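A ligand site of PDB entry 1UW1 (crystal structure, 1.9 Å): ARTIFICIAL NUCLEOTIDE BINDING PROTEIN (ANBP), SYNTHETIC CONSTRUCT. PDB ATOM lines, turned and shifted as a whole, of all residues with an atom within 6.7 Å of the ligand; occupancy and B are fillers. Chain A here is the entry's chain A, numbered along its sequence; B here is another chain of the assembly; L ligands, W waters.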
ATOM      1  N   VAL A  26       9.941 -17.826 -19.851  1.00  0.00           N
ATOM      2  CA  VAL A  26       9.901 -17.557 -21.279  1.00  0.00           C
ATOM      3  C   VAL A  26      10.862 -16.404 -21.704  1.00  0.00           C
ATOM      4  O   VAL A  26      11.238 -16.314 -22.850  1.00  0.00           O
ATOM      5  CB  VAL A  26       8.474 -17.203 -21.785  1.00  0.00           C
ATOM      6  CG1 VAL A  26       7.518 -18.292 -21.526  1.00  0.00           C
ATOM      7  CG2 VAL A  26       7.967 -15.872 -21.215  1.00  0.00           C
ATOM      8  N   ARG A  33       9.669 -20.791 -13.487  1.00  0.00           N
ATOM      9  CA  ARG A  33       8.590 -19.835 -13.438  1.00  0.00           C
ATOM     10  C   ARG A  33       8.062 -19.514 -12.041  1.00  0.00           C
ATOM     11  O   ARG A  33       8.103 -20.338 -11.138  1.00  0.00           O
ATOM     12  CB  ARG A  33       7.437 -20.302 -14.343  1.00  0.00           C
ATOM     13  CG  ARG A  33       7.850 -20.448 -15.783  1.00  0.00           C
ATOM     14  CD  ARG A  33       6.843 -21.141 -16.687  1.00  0.00           C
ATOM     15  NE  ARG A  33       7.347 -21.180 -18.048  1.00  0.00           N
ATOM     16  CZ  ARG A  33       6.616 -20.969 -19.150  1.00  0.00           C
ATOM     17  NH1 ARG A  33       5.334 -20.768 -19.099  1.00  0.00           N
ATOM     18  NH2 ARG A  33       7.188 -21.057 -20.305  1.00  0.00           N
ATOM     19  N   ASN A  34       7.540 -18.300 -11.853  1.00  0.00           N
ATOM     20  CA  ASN A  34       6.783 -18.015 -10.685  1.00  0.00           C
ATOM     21  C   ASN A  34       5.467 -18.749 -10.816  1.00  0.00           C
ATOM     22  O   ASN A  34       5.045 -19.126 -11.914  1.00  0.00           O
ATOM     23  CB  ASN A  34       6.575 -16.553 -10.487  1.00  0.00           C
ATOM     24  CG  ASN A  34       6.160 -16.220  -9.083  1.00  0.00           C
ATOM     25  OD1 ASN A  34       6.517 -16.914  -8.119  1.00  0.00           O
ATOM     26  ND2 ASN A  34       5.444 -15.127  -8.955  1.00  0.00           N
ATOM     27  N   TRP A  35       4.858 -18.957  -9.665  1.00  0.00           N
ATOM     28  CA  TRP A  35       3.620 -19.702  -9.522  1.00  0.00           C
ATOM     29  C   TRP A  35       2.923 -19.325  -8.231  1.00  0.00           C
ATOM     30  O   TRP A  35       3.484 -18.691  -7.378  1.00  0.00           O
ATOM     31  CB  TRP A  35       3.944 -21.193  -9.525  1.00  0.00           C
ATOM     32  CG  TRP A  35       4.863 -21.593  -8.414  1.00  0.00           C
ATOM     33  CD1 TRP A  35       6.229 -21.496  -8.388  1.00  0.00           C
ATOM     34  CD2 TRP A  35       4.469 -22.122  -7.163  1.00  0.00           C
ATOM     35  NE1 TRP A  35       6.704 -21.900  -7.170  1.00  0.00           N
ATOM     36  CE2 TRP A  35       5.654 -22.318  -6.404  1.00  0.00           C
ATOM     37  CE3 TRP A  35       3.249 -22.423  -6.583  1.00  0.00           C
ATOM     38  CZ2 TRP A  35       5.631 -22.831  -5.127  1.00  0.00           C
ATOM     39  CZ3 TRP A  35       3.228 -22.964  -5.278  1.00  0.00           C
ATOM     40  CH2 TRP A  35       4.437 -23.134  -4.566  1.00  0.00           C
ATOM     41  N   LYS A  36       1.674 -19.704  -8.095  1.00  0.00           N
ATOM     42  CA  LYS A  36       0.996 -19.542  -6.855  1.00  0.00           C
ATOM     43  C   LYS A  36      -0.128 -20.560  -6.788  1.00  0.00           C
ATOM     44  O   LYS A  36      -0.563 -21.039  -7.804  1.00  0.00           O
ATOM     45  CB  LYS A  36       0.462 -18.120  -6.667  1.00  0.00           C
ATOM     46  CG  LYS A  36      -0.807 -17.761  -7.366  1.00  0.00           C
ATOM     47  CD  LYS A  36      -1.389 -16.423  -6.886  1.00  0.00           C
ATOM     48  CE  LYS A  36      -2.558 -16.002  -7.800  1.00  0.00           C
ATOM     49  NZ  LYS A  36      -3.155 -14.601  -7.602  1.00  0.00           N
ATOM     50  N   LYS A  38      -3.925 -21.063  -5.972  1.00  0.00           N
ATOM     51  CA  LYS A  38      -5.178 -20.373  -5.772  1.00  0.00           C
ATOM     52  C   LYS A  38      -6.349 -21.332  -5.756  1.00  0.00           C
ATOM     53  O   LYS A  38      -6.757 -21.875  -6.783  1.00  0.00           O
ATOM     54  CB  LYS A  38      -5.378 -19.232  -6.754  1.00  0.00           C
ATOM     55  CG  LYS A  38      -5.306 -19.543  -8.231  1.00  0.00           C
ATOM     56  CD  LYS A  38      -5.415 -18.226  -9.019  1.00  0.00           C
ATOM     57  CE  LYS A  38      -6.744 -17.472  -8.834  1.00  0.00           C
ATOM     58  NZ  LYS A  38      -6.571 -16.012  -8.501  1.00  0.00           N
ATOM     59  N   ARG A  43      -1.434 -21.967 -10.385  1.00  0.00           N
ATOM     60  CA  ARG A  43      -1.189 -20.987 -11.459  1.00  0.00           C
ATOM     61  C   ARG A  43       0.271 -20.913 -11.739  1.00  0.00           C
ATOM     62  O   ARG A  43       1.035 -20.600 -10.858  1.00  0.00           O
ATOM     63  CB  ARG A  43      -1.690 -19.600 -11.048  1.00  0.00           C
ATOM     64  CG  ARG A  43      -1.445 -18.525 -12.052  1.00  0.00           C
ATOM     65  CD  ARG A  43      -2.282 -17.287 -11.880  1.00  0.00           C
ATOM     66  NE  ARG A  43      -3.657 -17.561 -12.222  1.00  0.00           N
ATOM     67  CZ  ARG A  43      -4.644 -16.696 -12.128  1.00  0.00           C
ATOM     68  NH1 ARG A  43      -4.430 -15.493 -11.690  1.00  0.00           N
ATOM     69  NH2 ARG A  43      -5.872 -17.060 -12.457  1.00  0.00           N
ATOM     70  N   TYR A  45       2.889 -18.912 -13.920  1.00  0.00           N
ATOM     71  CA  TYR A  45       3.080 -17.707 -14.726  1.00  0.00           C
ATOM     72  C   TYR A  45       4.125 -17.915 -15.772  1.00  0.00           C
ATOM     73  O   TYR A  45       4.926 -18.828 -15.673  1.00  0.00           O
ATOM     74  CB  TYR A  45       3.460 -16.543 -13.829  1.00  0.00           C
ATOM     75  CG  TYR A  45       2.449 -16.165 -12.781  1.00  0.00           C
ATOM     76  CD1 TYR A  45       1.349 -15.384 -13.103  1.00  0.00           C
ATOM     77  CD2 TYR A  45       2.637 -16.511 -11.471  1.00  0.00           C
ATOM     78  CE1 TYR A  45       0.460 -15.004 -12.146  1.00  0.00           C
ATOM     79  CE2 TYR A  45       1.763 -16.161 -10.531  1.00  0.00           C
ATOM     80  CZ  TYR A  45       0.666 -15.426 -10.859  1.00  0.00           C
ATOM     81  OH  TYR A  45      -0.217 -15.113  -9.857  1.00  0.00           O
ATOM     82  N   ASN A  46       4.182 -17.004 -16.764  1.00  0.00           N
ATOM     83  CA  ASN A  46       5.050 -17.245 -17.908  1.00  0.00           C
ATOM     84  C   ASN A  46       6.516 -16.981 -17.538  1.00  0.00           C
ATOM     85  O   ASN A  46       7.411 -17.513 -18.132  1.00  0.00           O
ATOM     86  CB  ASN A  46       4.696 -16.404 -19.137  1.00  0.00           C
ATOM     87  CG  ASN A  46       3.393 -16.817 -19.832  1.00  0.00           C
ATOM     88  OD1 ASN A  46       2.868 -17.912 -19.676  1.00  0.00           O
ATOM     89  ND2 ASN A  46       2.861 -15.887 -20.596  1.00  0.00           N
ATOM     90  N   MET A  47       6.749 -16.128 -16.567  1.00  0.00           N
ATOM     91  CA  MET A  47       8.092 -15.700 -16.222  1.00  0.00           C
ATOM     92  C   MET A  47       8.422 -15.938 -14.778  1.00  0.00           C
ATOM     93  O   MET A  47       7.552 -16.080 -13.963  1.00  0.00           O
ATOM     94  CB  MET A  47       8.333 -14.213 -16.488  1.00  0.00           C
ATOM     95  CG  MET A  47       8.325 -13.815 -17.956  1.00  0.00           C
ATOM     96  SD  MET A  47       8.606 -12.049 -18.221  1.00  0.00           S
ATOM     97  CE  MET A  47       7.020 -11.460 -17.847  1.00  0.00           C
ATOM     98  N   CYS A  48       9.724 -15.921 -14.499  1.00  0.00           N
ATOM     99  CA  CYS A  48      10.218 -15.976 -13.132  1.00  0.00           C
ATOM    100  C   CYS A  48       9.938 -14.625 -12.496  1.00  0.00           C
ATOM    101  O   CYS A  48       9.466 -13.727 -13.181  1.00  0.00           O
ATOM    102  CB  CYS A  48      11.722 -16.252 -13.100  1.00  0.00           C
ATOM    103  SG  CYS A  48      12.831 -15.015 -13.706  1.00  0.00           S
ATOM    104  N   LYS A  49      10.123 -14.532 -11.190  1.00  0.00           N
ATOM    105  CA  LYS A  49       9.810 -13.300 -10.473  1.00  0.00           C
ATOM    106  C   LYS A  49      10.743 -12.139 -10.916  1.00  0.00           C
ATOM    107  O   LYS A  49      10.282 -11.042 -11.146  1.00  0.00           O
ATOM    108  CB  LYS A  49       9.861 -13.524  -8.984  1.00  0.00           C
ATOM    109  CG  LYS A  49       9.546 -12.247  -8.161  1.00  0.00           C
ATOM    110  CD  LYS A  49       8.126 -11.806  -8.329  1.00  0.00           C
ATOM    111  CE  LYS A  49       7.792 -10.812  -7.208  1.00  0.00           C
ATOM    112  NZ  LYS A  49       6.353 -10.692  -6.973  1.00  0.00           N
ATOM    113  N   CYS A  51      12.323 -11.635 -13.886  1.00  0.00           N
ATOM    114  CA  CYS A  51      11.934 -11.165 -15.228  1.00  0.00           C
ATOM    115  C   CYS A  51      10.570 -10.424 -15.230  1.00  0.00           C
ATOM    116  O   CYS A  51      10.409  -9.380 -15.851  1.00  0.00           O
ATOM    117  CB  CYS A  51      11.985 -12.334 -16.228  1.00  0.00           C
ATOM    118  SG  CYS A  51      13.673 -12.834 -16.614  1.00  0.00           S
ATOM    119  N   PHE A  52       9.589 -10.922 -14.479  1.00  0.00           N
ATOM    120  CA  PHE A  52       8.322 -10.230 -14.334  1.00  0.00           C
ATOM    121  C   PHE A  52       8.513  -8.857 -13.715  1.00  0.00           C
ATOM    122  O   PHE A  52       8.022  -7.884 -14.276  1.00  0.00           O
ATOM    123  CB  PHE A  52       7.304 -11.045 -13.566  1.00  0.00           C
ATOM    124  CG  PHE A  52       5.999 -10.320 -13.355  1.00  0.00           C
ATOM    125  CD1 PHE A  52       5.137 -10.104 -14.415  1.00  0.00           C
ATOM    126  CD2 PHE A  52       5.665  -9.830 -12.111  1.00  0.00           C
ATOM    127  CE1 PHE A  52       3.934  -9.409 -14.213  1.00  0.00           C
ATOM    128  CE2 PHE A  52       4.483  -9.166 -11.913  1.00  0.00           C
ATOM    129  CZ  PHE A  52       3.634  -8.933 -12.985  1.00  0.00           C
ATOM    130  N   ASN A  53       9.233  -8.724 -12.599  1.00  0.00           N
ATOM    131  CA  ASN A  53       9.435  -7.403 -12.036  1.00  0.00           C
ATOM    132  C   ASN A  53      10.145  -6.485 -13.071  1.00  0.00           C
ATOM    133  O   ASN A  53       9.821  -5.349 -13.194  1.00  0.00           O
ATOM    134  CB  ASN A  53      10.240  -7.435 -10.780  1.00  0.00           C
ATOM    135  CG  ASN A  53       9.440  -7.953  -9.551  1.00  0.00           C
ATOM    136  OD1 ASN A  53       8.231  -7.993  -9.540  1.00  0.00           O
ATOM    137  ND2 ASN A  53      10.164  -8.342  -8.564  1.00  0.00           N
ATOM    138  N   SER A  55       9.962  -6.707 -16.356  1.00  0.00           N
ATOM    139  CA  SER A  55       9.038  -6.368 -17.401  1.00  0.00           C
ATOM    140  C   SER A  55       8.223  -5.144 -17.070  1.00  0.00           C
ATOM    141  O   SER A  55       7.908  -4.391 -17.945  1.00  0.00           O
ATOM    142  CB  SER A  55       8.093  -7.512 -17.794  1.00  0.00           C
ATOM    143  OG  SER A  55       7.167  -7.792 -16.760  1.00  0.00           O
ATOM    144  N   TYR A  63       5.265 -10.747 -22.457  1.00  0.00           N
ATOM    145  CA  TYR A  63       5.348 -12.051 -21.858  1.00  0.00           C
ATOM    146  C   TYR A  63       4.503 -12.234 -20.610  1.00  0.00           C
ATOM    147  O   TYR A  63       4.630 -13.269 -19.919  1.00  0.00           O
ATOM    148  CB  TYR A  63       6.841 -12.383 -21.579  1.00  0.00           C
ATOM    149  CG  TYR A  63       7.623 -12.276 -22.846  1.00  0.00           C
ATOM    150  CD1 TYR A  63       7.532 -13.270 -23.798  1.00  0.00           C
ATOM    151  CD2 TYR A  63       8.379 -11.124 -23.159  1.00  0.00           C
ATOM    152  CE1 TYR A  63       8.189 -13.159 -25.010  1.00  0.00           C
ATOM    153  CE2 TYR A  63       9.030 -10.988 -24.358  1.00  0.00           C
ATOM    154  CZ  TYR A  63       8.935 -12.023 -25.282  1.00  0.00           C
ATOM    155  OH  TYR A  63       9.560 -11.938 -26.490  1.00  0.00           O
ATOM    156  N   HIS A  64       3.604 -11.315 -20.349  1.00  0.00           N
ATOM    157  CA  HIS A  64       2.647 -11.489 -19.244  1.00  0.00           C
ATOM    158  C   HIS A  64       1.660 -12.582 -19.569  1.00  0.00           C
ATOM    159  O   HIS A  64       1.222 -12.706 -20.690  1.00  0.00           O
ATOM    160  CB  HIS A  64       1.916 -10.222 -18.946  1.00  0.00           C
ATOM    161  CG  HIS A  64       2.759  -9.164 -18.346  1.00  0.00           C
ATOM    162  ND1 HIS A  64       2.262  -7.997 -17.818  1.00  0.00           N
ATOM    163  CD2 HIS A  64       4.098  -9.114 -18.165  1.00  0.00           C
ATOM    164  CE1 HIS A  64       3.259  -7.274 -17.333  1.00  0.00           C
ATOM    165  NE2 HIS A  64       4.393  -7.916 -17.577  1.00  0.00           N
ATOM    166  N   GLY A  65       1.312 -13.385 -18.564  1.00  0.00           N
ATOM    167  CA  GLY A  65       0.378 -14.474 -18.756  1.00  0.00           C
ATOM    168  C   GLY A  65       0.619 -15.618 -17.808  1.00  0.00           C
ATOM    169  O   GLY A  65       1.588 -15.663 -17.111  1.00  0.00           O
ATOM    170  N   HIS A  66      -0.256 -16.600 -17.891  1.00  0.00           N
ATOM    171  CA  HIS A  66      -0.220 -17.749 -17.024  1.00  0.00           C
ATOM    172  C   HIS A  66      -1.121 -18.824 -17.508  1.00  0.00           C
ATOM    173  O   HIS A  66      -1.939 -18.596 -18.384  1.00  0.00           O
ATOM    174  CB  HIS A  66      -0.681 -17.375 -15.604  1.00  0.00           C
ATOM    175  CG  HIS A  66      -2.082 -16.843 -15.533  1.00  0.00           C
ATOM    176  ND1 HIS A  66      -2.369 -15.509 -15.421  1.00  0.00           N
ATOM    177  CD2 HIS A  66      -3.272 -17.487 -15.548  1.00  0.00           C
ATOM    178  CE1 HIS A  66      -3.680 -15.343 -15.377  1.00  0.00           C
ATOM    179  NE2 HIS A  66      -4.242 -16.530 -15.445  1.00  0.00           N
ATOM    180  N   ASP B  74      -7.211 -20.143 -17.900  1.00  0.00           N
ATOM    181  CA  ASP B  74      -7.653 -19.465 -16.669  1.00  0.00           C
ATOM    182  C   ASP B  74      -8.811 -20.139 -15.919  1.00  0.00           C
ATOM    183  O   ASP B  74      -9.883 -20.363 -16.457  1.00  0.00           O
ATOM    184  CB  ASP B  74      -8.002 -18.015 -16.984  1.00  0.00           C
ATOM    185  CG  ASP B  74      -7.874 -17.132 -15.788  1.00  0.00           C
ATOM    186  OD1 ASP B  74      -8.678 -17.311 -14.828  1.00  0.00           O
ATOM    187  OD2 ASP B  74      -6.988 -16.243 -15.702  1.00  0.00           O
HETATM  188  P1  LIG L   1      -5.287 -12.425 -10.160  1.00  0.00           P
HETATM  189  O1  LIG L   1      -5.817 -11.126  -9.637  1.00  0.00           O
HETATM  190  O2  LIG L   1      -4.974 -13.399  -8.980  1.00  0.00           O
HETATM  191  O3  LIG L   1      -6.328 -13.115 -11.088  1.00  0.00           O
HETATM  192  P2  LIG L   1      -2.538 -12.413 -10.868  1.00  0.00           P
HETATM  193  O4  LIG L   1      -1.963 -11.573  -9.785  1.00  0.00           O
HETATM  194  O5  LIG L   1      -2.373 -13.910 -10.679  1.00  0.00           O
HETATM  195  O6  LIG L   1      -4.064 -11.983 -11.100  1.00  0.00           O
HETATM  196  O7  LIG L   1      -1.932 -11.972 -12.267  1.00  0.00           O
HETATM  197  C1  LIG L   1      -1.979 -10.616 -12.683  1.00  0.00           C
HETATM  198  C2  LIG L   1      -1.530 -10.445 -14.139  1.00  0.00           C
HETATM  199  O8  LIG L   1      -0.114 -10.379 -14.207  1.00  0.00           O
HETATM  200  C3  LIG L   1      -1.899 -11.589 -15.031  1.00  0.00           C
HETATM  201  O9  LIG L   1      -2.071 -11.191 -16.374  1.00  0.00           O
HETATM  202  C4  LIG L   1      -0.670 -12.470 -14.922  1.00  0.00           C
HETATM  203  O10 LIG L   1      -0.592 -13.307 -15.994  1.00  0.00           O
HETATM  204  C5  LIG L   1       0.460 -11.454 -14.876  1.00  0.00           C
HETATM  205  N1  LIG L   1       1.629 -11.970 -14.133  1.00  0.00           N
HETATM  206  C6  LIG L   1       1.808 -11.939 -12.760  1.00  0.00           C
HETATM  207  N2  LIG L   1       3.008 -12.519 -12.494  1.00  0.00           N
HETATM  208  C7  LIG L   1       3.566 -12.884 -13.692  1.00  0.00           C
HETATM  209  C8  LIG L   1       4.740 -13.499 -13.998  1.00  0.00           C
HETATM  210  N3  LIG L   1       5.565 -13.919 -13.019  1.00  0.00           N
HETATM  211  N4  LIG L   1       4.998 -13.755 -15.326  1.00  0.00           N
HETATM  212  C9  LIG L   1       4.148 -13.398 -16.355  1.00  0.00           C
HETATM  213  N5  LIG L   1       2.968 -12.774 -16.069  1.00  0.00           N
HETATM  214  C10 LIG L   1       2.706 -12.538 -14.733  1.00  0.00           C
HETATM  215  O   HOH W   1      -5.621  -9.603 -11.792  1.00  0.00           O
HETATM  216  O   HOH W   2      -5.382 -12.430 -13.440  1.00  0.00           O
HETATM  217  O   HOH W   3      -2.951 -12.771 -18.129  1.00  0.00           O
HETATM  218  O   HOH W   4       4.591 -12.870 -10.367  1.00  0.00           O
HETATM  219  O   HOH W   5       0.549 -10.356 -10.113  1.00  0.00           O
HETATM  220  O   HOH W   6      -1.496 -12.633  -7.557  1.00  0.00           O
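A nitrogen (N5) of the ligand lies within hydrogen-bond range of the backbone NH of Gly 65 (3.1 Å).
The side-chain hydroxyl (OH) of Tyr 45 lies within hydrogen-bond range of an oxygen (O5) of the ligand (2.6 Å).
O of Gly 65 sits close to O10 of the ligand.
N of Met 47 sits at hydrogen-bond distance from N4 of the ligand, 3.2 Å away.
The side-chain amino group (NZ) of Lys 38 lies within salt-bridge range of an oxygen (O2) of the ligand.
O of Met 47 is in hydrogen-bond range of N3 of the ligand.
O2 of the ligand lies within salt-bridge range of NZ of Lys 36 (2.6 Å).
ND1 of His 66 lies within hydrogen-bond range of O10 of the ligand, 2.9 Å away.
The guanidinium group (NH1) of Arg 43 is in salt-bridge range of an oxygen (O5) of the ligand (2.8 Å).
The side-chain carboxylate of Asp 74 of chain B lies within hydrogen-bond range of a ring nitrogen (NE2) of His 66 (2.8 Å).
The backbone NH (N) of Tyr 45 lies within hydrogen-bond range of the backbone carbonyl oxygen (O) of Asn 34.
NE of Arg 43 sits close to NE2 of His 66 (3.4 Å).
O of Gly 65 lies within hydrogen-bond range of N of Asn 46 (2.9 Å).
The backbone NH of Asn 34 is in hydrogen-bond range of the backbone carbonyl oxygen of Met 47 (3.1 Å).
The guanidinium group (NH2) of Arg 43 lies within salt-bridge range of the side-chain carboxylate (OD2) of Asp 74 of chain B (3.5 Å).
O of Phe 52 sits at hydrogen-bond distance from OG of Ser 55, 2.6 Å away.
NE2 of His 64 lies within hydrogen-bond range of OG of Ser 55.
Merely in contact with the ligand: Asn 34 (3.8 Å), Asn 46 (3.6 Å), Cys 48 (3.9 Å), Phe 52 (3.3 Å), Tyr 63 (3.6 Å) and His 64 (3.4 Å).
Hydrophobic or aromatic side chains within 4 Å of the ligand: Tyr 45, Met 47, Phe 52, His 64 and His 66.
13 residues have an atom within 4 Å of the ligand: Asn 34, Lys 36, Lys 38, Arg 43, Tyr 45, Asn 46, Met 47, Cys 48, Phe 52, Tyr 63, His 64, Gly 65 and His 66.
Water W6 bridges O4 of the ligand (2.5 Å) and NZ of Lys 36 (2.6 Å).
Water W4 lies within hydrogen-bond range of a nitrogen (N2) of the ligand and the side-chain amide nitrogen of Asn 34.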
